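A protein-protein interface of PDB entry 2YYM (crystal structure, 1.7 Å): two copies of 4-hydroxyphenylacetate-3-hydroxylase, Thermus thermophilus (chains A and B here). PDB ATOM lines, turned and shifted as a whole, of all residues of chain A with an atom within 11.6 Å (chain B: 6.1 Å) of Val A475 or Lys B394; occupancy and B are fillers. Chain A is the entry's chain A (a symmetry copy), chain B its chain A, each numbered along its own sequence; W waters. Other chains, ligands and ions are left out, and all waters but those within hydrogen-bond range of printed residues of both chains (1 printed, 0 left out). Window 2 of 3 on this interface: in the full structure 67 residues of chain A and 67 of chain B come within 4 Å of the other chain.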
ATOM      1  N   ALA A 467      -3.894  23.132  11.206  1.00  0.00           N
ATOM      2  CA  ALA A 467      -5.211  23.411  10.643  1.00  0.00           C
ATOM      3  C   ALA A 467      -6.231  22.416  11.181  1.00  0.00           C
ATOM      4  O   ALA A 467      -7.357  22.784  11.513  1.00  0.00           O
ATOM      5  CB  ALA A 467      -5.165  23.335   9.118  1.00  0.00           C
ATOM      6  N   PHE A 468      -5.838  21.149  11.268  1.00  0.00           N
ATOM      7  CA  PHE A 468      -6.746  20.120  11.763  1.00  0.00           C
ATOM      8  C   PHE A 468      -7.095  20.352  13.230  1.00  0.00           C
ATOM      9  O   PHE A 468      -8.214  20.067  13.664  1.00  0.00           O
ATOM     10  CB  PHE A 468      -6.117  18.729  11.622  1.00  0.00           C
ATOM     11  CG  PHE A 468      -7.106  17.609  11.761  1.00  0.00           C
ATOM     12  CD1 PHE A 468      -7.846  17.185  10.663  1.00  0.00           C
ATOM     13  CD2 PHE A 468      -7.335  17.010  12.997  1.00  0.00           C
ATOM     14  CE1 PHE A 468      -8.801  16.179  10.793  1.00  0.00           C
ATOM     15  CE2 PHE A 468      -8.288  16.005  13.138  1.00  0.00           C
ATOM     16  CZ  PHE A 468      -9.022  15.589  12.034  1.00  0.00           C
ATOM     17  N   LEU A 469      -6.137  20.871  13.990  1.00  0.00           N
ATOM     18  CA  LEU A 469      -6.338  21.114  15.410  1.00  0.00           C
ATOM     19  C   LEU A 469      -7.143  22.373  15.734  1.00  0.00           C
ATOM     20  O   LEU A 469      -7.500  22.597  16.888  1.00  0.00           O
ATOM     21  CB  LEU A 469      -4.984  21.170  16.128  1.00  0.00           C
ATOM     22  CG  LEU A 469      -4.180  19.859  16.130  1.00  0.00           C
ATOM     23  CD1 LEU A 469      -2.821  20.084  16.779  1.00  0.00           C
ATOM     24  CD2 LEU A 469      -4.958  18.781  16.879  1.00  0.00           C
ATOM     25  N   LYS A 470      -7.430  23.194  14.729  1.00  0.00           N
ATOM     26  CA  LYS A 470      -8.209  24.411  14.971  1.00  0.00           C
ATOM     27  C   LYS A 470      -9.544  24.052  15.614  1.00  0.00           C
ATOM     28  O   LYS A 470     -10.025  24.753  16.507  1.00  0.00           O
ATOM     29  CB  LYS A 470      -8.454  25.164  13.659  1.00  0.00           C
ATOM     30  CG  LYS A 470      -7.194  25.711  13.012  1.00  0.00           C
ATOM     31  CD  LYS A 470      -6.526  26.761  13.884  1.00  0.00           C
ATOM     32  CE  LYS A 470      -5.283  27.328  13.204  1.00  0.00           C
ATOM     33  NZ  LYS A 470      -4.647  28.419  13.994  1.00  0.00           N
ATOM     34  N   GLU A 471     -10.132  22.951  15.160  1.00  0.00           N
ATOM     35  CA  GLU A 471     -11.412  22.495  15.689  1.00  0.00           C
ATOM     36  C   GLU A 471     -11.279  22.099  17.158  1.00  0.00           C
ATOM     37  O   GLU A 471     -12.221  22.241  17.942  1.00  0.00           O
ATOM     38  CB  GLU A 471     -11.918  21.306  14.874  1.00  0.00           C
ATOM     39  CG  GLU A 471     -13.399  21.036  15.030  1.00  0.00           C
ATOM     40  CD  GLU A 471     -14.248  22.231  14.638  1.00  0.00           C
ATOM     41  OE1 GLU A 471     -14.020  22.788  13.543  1.00  0.00           O
ATOM     42  OE2 GLU A 471     -15.145  22.609  15.422  1.00  0.00           O
ATOM     43  N   SER A 472     -10.107  21.593  17.529  1.00  0.00           N
ATOM     44  CA  SER A 472      -9.854  21.192  18.905  1.00  0.00           C
ATOM     45  C   SER A 472      -9.834  22.413  19.821  1.00  0.00           C
ATOM     46  O   SER A 472     -10.485  22.427  20.862  1.00  0.00           O
ATOM     47  CB  SER A 472      -8.509  20.463  19.013  1.00  0.00           C
ATOM     48  OG  SER A 472      -8.521  19.246  18.284  1.00  0.00           O
ATOM     49  N   LEU A 473      -9.085  23.437  19.426  1.00  0.00           N
ATOM     50  CA  LEU A 473      -8.972  24.650  20.231  1.00  0.00           C
ATOM     51  C   LEU A 473     -10.242  25.495  20.251  1.00  0.00           C
ATOM     52  O   LEU A 473     -10.417  26.340  21.129  1.00  0.00           O
ATOM     53  CB  LEU A 473      -7.797  25.501  19.738  1.00  0.00           C
ATOM     54  CG  LEU A 473      -6.382  24.963  20.001  1.00  0.00           C
ATOM     55  CD1 LEU A 473      -6.164  24.805  21.499  1.00  0.00           C
ATOM     56  CD2 LEU A 473      -6.189  23.637  19.299  1.00  0.00           C
ATOM     57  N   LYS A 474     -11.130  25.261  19.293  1.00  0.00           N
ATOM     58  CA  LYS A 474     -12.372  26.020  19.216  1.00  0.00           C
ATOM     59  C   LYS A 474     -13.320  25.750  20.388  1.00  0.00           C
ATOM     60  O   LYS A 474     -14.232  26.537  20.639  1.00  0.00           O
ATOM     61  CB  LYS A 474     -13.084  25.717  17.895  1.00  0.00           C
ATOM     62  CG  LYS A 474     -14.284  26.605  17.615  1.00  0.00           C
ATOM     63  CD  LYS A 474     -14.892  26.314  16.251  1.00  0.00           C
ATOM     64  CE  LYS A 474     -16.073  27.233  15.972  1.00  0.00           C
ATOM     65  NZ  LYS A 474     -16.713  26.937  14.657  1.00  0.00           N
ATOM     66  N   VAL A 475     -13.109  24.648  21.104  1.00  0.00           N
ATOM     67  CA  VAL A 475     -13.973  24.307  22.231  1.00  0.00           C
ATOM     68  C   VAL A 475     -13.833  25.287  23.388  1.00  0.00           C
ATOM     69  O   VAL A 475     -14.675  25.321  24.288  1.00  0.00           O
ATOM     70  CB  VAL A 475     -13.685  22.880  22.772  1.00  0.00           C
ATOM     71  CG1 VAL A 475     -13.858  21.851  21.657  1.00  0.00           C
ATOM     72  CG2 VAL A 475     -12.284  22.814  23.370  1.00  0.00           C
ATOM     73  N   PHE A 476     -12.770  26.084  23.368  1.00  0.00           N
ATOM     74  CA  PHE A 476     -12.544  27.048  24.438  1.00  0.00           C
ATOM     75  C   PHE A 476     -13.078  28.432  24.104  1.00  0.00           C
ATOM     76  O   PHE A 476     -13.091  29.315  24.962  1.00  0.00           O
ATOM     77  CB  PHE A 476     -11.050  27.140  24.769  1.00  0.00           C
ATOM     78  CG  PHE A 476     -10.441  25.831  25.177  1.00  0.00           C
ATOM     79  CD1 PHE A 476      -9.536  25.184  24.342  1.00  0.00           C
ATOM     80  CD2 PHE A 476     -10.785  25.235  26.385  1.00  0.00           C
ATOM     81  CE1 PHE A 476      -8.980  23.956  24.705  1.00  0.00           C
ATOM     82  CE2 PHE A 476     -10.235  24.007  26.758  1.00  0.00           C
ATOM     83  CZ  PHE A 476      -9.331  23.366  25.916  1.00  0.00           C
ATOM     84  N   GLU A 477     -13.516  28.621  22.861  1.00  0.00           N
ATOM     85  CA  GLU A 477     -14.049  29.916  22.435  1.00  0.00           C
ATOM     86  C   GLU A 477     -15.402  30.189  23.070  1.00  0.00           C
ATOM     87  O   GLU A 477     -16.048  29.231  23.552  1.00  0.00           O
ATOM     88  CB  GLU A 477     -14.211  29.977  20.918  1.00  0.00           C
ATOM     89  CG  GLU A 477     -12.910  29.834  20.153  1.00  0.00           C
ATOM     90  CD  GLU A 477     -13.064  30.171  18.687  1.00  0.00           C
ATOM     91  OE1 GLU A 477     -14.171  29.947  18.147  1.00  0.00           O
ATOM     92  OE2 GLU A 477     -12.086  30.646  18.059  1.00  0.00           O
ATOM     93  N   SER B 233     -16.336  15.462  21.837  1.00  0.00           N
ATOM     94  CA  SER B 233     -15.436  16.606  21.916  1.00  0.00           C
ATOM     95  C   SER B 233     -14.289  16.472  20.918  1.00  0.00           C
ATOM     96  O   SER B 233     -13.583  15.467  20.907  1.00  0.00           O
ATOM     97  CB  SER B 233     -14.861  16.738  23.326  1.00  0.00           C
ATOM     98  OG  SER B 233     -13.848  17.735  23.359  1.00  0.00           O
ATOM     99  N   PRO B 234     -14.103  17.480  20.054  1.00  0.00           N
ATOM    100  CA  PRO B 234     -13.010  17.408  19.079  1.00  0.00           C
ATOM    101  C   PRO B 234     -11.659  17.586  19.771  1.00  0.00           C
ATOM    102  O   PRO B 234     -10.631  17.137  19.268  1.00  0.00           O
ATOM    103  CB  PRO B 234     -13.338  18.541  18.106  1.00  0.00           C
ATOM    104  CG  PRO B 234     -14.064  19.531  18.974  1.00  0.00           C
ATOM    105  CD  PRO B 234     -14.970  18.642  19.789  1.00  0.00           C
ATOM    106  N   PHE B 235     -11.660  18.247  20.926  1.00  0.00           N
ATOM    107  CA  PHE B 235     -10.422  18.448  21.675  1.00  0.00           C
ATOM    108  C   PHE B 235     -10.005  17.123  22.310  1.00  0.00           C
ATOM    109  O   PHE B 235      -8.863  16.690  22.172  1.00  0.00           O
ATOM    110  CB  PHE B 235     -10.617  19.491  22.785  1.00  0.00           C
ATOM    111  CG  PHE B 235      -9.369  19.758  23.589  1.00  0.00           C
ATOM    112  CD1 PHE B 235      -8.482  20.764  23.211  1.00  0.00           C
ATOM    113  CD2 PHE B 235      -9.075  18.997  24.717  1.00  0.00           C
ATOM    114  CE1 PHE B 235      -7.319  21.011  23.946  1.00  0.00           C
ATOM    115  CE2 PHE B 235      -7.913  19.235  25.458  1.00  0.00           C
ATOM    116  CZ  PHE B 235      -7.037  20.246  25.071  1.00  0.00           C
ATOM    117  N   SER B 389      -8.658  16.581  30.128  1.00  0.00           N
ATOM    118  CA  SER B 389      -9.741  16.936  29.219  1.00  0.00           C
ATOM    119  C   SER B 389      -9.906  18.442  29.066  1.00  0.00           C
ATOM    120  O   SER B 389      -9.378  19.219  29.862  1.00  0.00           O
ATOM    121  CB  SER B 389     -11.055  16.343  29.738  1.00  0.00           C
ATOM    122  OG  SER B 389     -12.172  16.866  29.039  1.00  0.00           O
ATOM    123  N   GLU B 390     -10.627  18.851  28.028  1.00  0.00           N
ATOM    124  CA  GLU B 390     -10.887  20.267  27.834  1.00  0.00           C
ATOM    125  C   GLU B 390     -11.630  20.706  29.096  1.00  0.00           C
ATOM    126  O   GLU B 390     -11.534  21.856  29.519  1.00  0.00           O
ATOM    127  CB  GLU B 390     -11.768  20.495  26.604  1.00  0.00           C
ATOM    128  CG  GLU B 390     -12.991  19.594  26.527  1.00  0.00           C
ATOM    129  CD  GLU B 390     -14.125  20.228  25.750  1.00  0.00           C
ATOM    130  OE1 GLU B 390     -14.655  21.257  26.222  1.00  0.00           O
ATOM    131  OE2 GLU B 390     -14.489  19.711  24.669  1.00  0.00           O
ATOM    132  N   LYS B 391     -12.351  19.764  29.701  1.00  0.00           N
ATOM    133  CA  LYS B 391     -13.113  20.038  30.919  1.00  0.00           C
ATOM    134  C   LYS B 391     -12.191  20.372  32.087  1.00  0.00           C
ATOM    135  O   LYS B 391     -12.558  21.143  32.977  1.00  0.00           O
ATOM    136  CB  LYS B 391     -13.997  18.843  31.279  1.00  0.00           C
ATOM    137  CG  LYS B 391     -15.169  18.633  30.337  1.00  0.00           C
ATOM    138  CD  LYS B 391     -16.092  17.541  30.851  1.00  0.00           C
ATOM    139  CE  LYS B 391     -17.334  17.406  29.981  1.00  0.00           C
ATOM    140  NZ  LYS B 391     -18.242  16.336  30.484  1.00  0.00           N
ATOM    141  N   ASP B 392     -10.996  19.786  32.092  1.00  0.00           N
ATOM    142  CA  ASP B 392     -10.041  20.072  33.155  1.00  0.00           C
ATOM    143  C   ASP B 392      -9.499  21.483  32.973  1.00  0.00           C
ATOM    144  O   ASP B 392      -9.297  22.211  33.948  1.00  0.00           O
ATOM    145  CB  ASP B 392      -8.895  19.063  33.136  1.00  0.00           C
ATOM    146  CG  ASP B 392      -9.336  17.689  33.572  1.00  0.00           C
ATOM    147  OD1 ASP B 392      -9.689  17.530  34.759  1.00  0.00           O
ATOM    148  OD2 ASP B 392      -9.335  16.771  32.727  1.00  0.00           O
ATOM    149  N   PHE B 393      -9.269  21.870  31.722  1.00  0.00           N
ATOM    150  CA  PHE B 393      -8.770  23.209  31.428  1.00  0.00           C
ATOM    151  C   PHE B 393      -9.827  24.254  31.760  1.00  0.00           C
ATOM    152  O   PHE B 393      -9.503  25.376  32.148  1.00  0.00           O
ATOM    153  CB  PHE B 393      -8.384  23.328  29.953  1.00  0.00           C
ATOM    154  CG  PHE B 393      -6.988  22.860  29.656  1.00  0.00           C
ATOM    155  CD1 PHE B 393      -5.893  23.592  30.096  1.00  0.00           C
ATOM    156  CD2 PHE B 393      -6.769  21.683  28.953  1.00  0.00           C
ATOM    157  CE1 PHE B 393      -4.592  23.160  29.842  1.00  0.00           C
ATOM    158  CE2 PHE B 393      -5.474  21.240  28.693  1.00  0.00           C
ATOM    159  CZ  PHE B 393      -4.384  21.980  29.138  1.00  0.00           C
ATOM    160  N   LYS B 394     -11.091  23.874  31.611  1.00  0.00           N
ATOM    161  CA  LYS B 394     -12.205  24.774  31.890  1.00  0.00           C
ATOM    162  C   LYS B 394     -12.579  24.773  33.370  1.00  0.00           C
ATOM    163  O   LYS B 394     -13.364  25.611  33.820  1.00  0.00           O
ATOM    164  CB  LYS B 394     -13.427  24.376  31.054  1.00  0.00           C
ATOM    165  CG  LYS B 394     -13.241  24.557  29.554  1.00  0.00           C
ATOM    166  CD  LYS B 394     -14.438  24.027  28.773  1.00  0.00           C
ATOM    167  CE  LYS B 394     -14.301  24.335  27.289  1.00  0.00           C
ATOM    168  NZ  LYS B 394     -15.467  23.833  26.503  1.00  0.00           N
ATOM    169  N   GLY B 395     -12.011  23.834  34.119  1.00  0.00           N
ATOM    170  CA  GLY B 395     -12.298  23.732  35.537  1.00  0.00           C
ATOM    171  C   GLY B 395     -11.353  24.511  36.437  1.00  0.00           C
ATOM    172  O   GLY B 395     -10.491  25.248  35.958  1.00  0.00           O
ATOM    173  N   PRO B 396     -11.494  24.354  37.763  1.00  0.00           N
ATOM    174  CA  PRO B 396     -10.698  25.010  38.808  1.00  0.00           C
ATOM    175  C   PRO B 396      -9.181  24.903  38.679  1.00  0.00           C
ATOM    176  O   PRO B 396      -8.458  25.843  39.015  1.00  0.00           O
ATOM    177  CB  PRO B 396     -11.205  24.348  40.085  1.00  0.00           C
ATOM    178  CG  PRO B 396     -12.634  24.071  39.762  1.00  0.00           C
ATOM    179  CD  PRO B 396     -12.540  23.511  38.367  1.00  0.00           C
ATOM    180  N   GLY B 398      -7.588  24.618  35.917  1.00  0.00           N
ATOM    181  CA  GLY B 398      -7.170  25.113  34.617  1.00  0.00           C
ATOM    182  C   GLY B 398      -5.861  25.883  34.664  1.00  0.00           C
ATOM    183  O   GLY B 398      -4.940  25.584  33.902  1.00  0.00           O
HETATM  184  O   HOH W   1      -7.158  17.513  20.001  1.00  0.00           O
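No position is printed for both chains.
Of the 11 pairs that touch across the chains among the printed residues, none has its exchanged pair printed and touching as well.
Among the printed residues, merely in contact across the chains: Glu A471 with Pro B234 (3.4 Å), Phe A476 with Phe B235 (3.5 Å), Ser A472 with Phe B235 (3.5 Å), Val A475 with Pro B234 (3.6 Å), Phe A476 with Glu B390 (3.7 Å), Phe A476 with Lys B394 (3.7 Å), Val A475 with Glu B390 (3.7 Å), Phe A476 with Phe B393 (3.8 Å) and Val A475 with Phe B235 (3.8 Å).
Of the 12 printed residues of chain B, 5 touch a printed residue of chain A.
Printed residues of chain B that touch a printed residue of chain A: Pro B234, Phe B235, Glu B390, Phe B393 and Lys B394.
Along chain B the printed residues that touch a printed residue of chain A span positions 234 to 394.
Printed residues of chain A that touch a printed residue of chain B: Glu A471, Ser A472, Val A475 and Phe A476.
Hydrophobic or aromatic side chains of chain A within 4 Å of the printed part of chain B: Val A475 and Phe A476.
The side-chain hydroxyl of Ser A472 is in hydrogen-bond range of the backbone carbonyl oxygen of Pro B234.
NZ of Lys B394 lies within hydrogen-bond range of O of Val A475 (2.8 Å).
The backbone NH of Phe B235 lies close to the side-chain hydroxyl of Ser B233, at 3.3 Å.
The side-chain hydroxyl (OG) of Ser B233 lies within hydrogen-bond range of the side-chain carboxylate (OE2) of Glu B390.
OE1 of Glu B390 lies within salt-bridge range of NZ of Lys B394, at 2.7 Å.
Of chain B, only Pro B234 (3.6 Å), Phe B235 (3.8 Å), Glu B390 (3.7 Å) and Lys B394 (2.8 Å) come within 4 Å of Val A475.
Lys B394 touches just these residues of chain A: Val A475 and Phe A476.
Printed residues of chain A within 4 Å of Pro B234: Glu A471 (3.4 Å), Ser A472 (3.1 Å) and Val A475 (3.6 Å).
Phe B235 touches just these residues of chain A: Ser A472 (3.5 Å), Val A475 (3.8 Å) and Phe A476 (3.5 Å).
Printed residues of chain A within 4 Å of Glu B390: Val A475 and Phe A476.
No residue of chain A comes within 4 Å of Asp B392.
Phe B393 touches just one residue of chain A: Phe A476.
No residue of chain A comes within 4 Å of Pro B396.
Of the printed residues of chain B, Glu A471 touches Pro B234.
Printed residues of chain B within 4 Å of Phe A476: Phe B235, Glu B390, Phe B393 and Lys B394.
Printed residues of chain B within 4 Å of Ser A472: Pro B234 (3.1 Å) and Phe B235 (3.5 Å).
The nearest residue of chain B that does not touch Val A475 is Ser B233 (4.5 Å).
The nearest printed residue of chain B that does not touch Glu A471 is Phe B235 (5.0 Å).
Water W1 lies within hydrogen-bond range of OG of Ser A472 (2.8 Å) and O of Phe B235 (2.9 Å).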
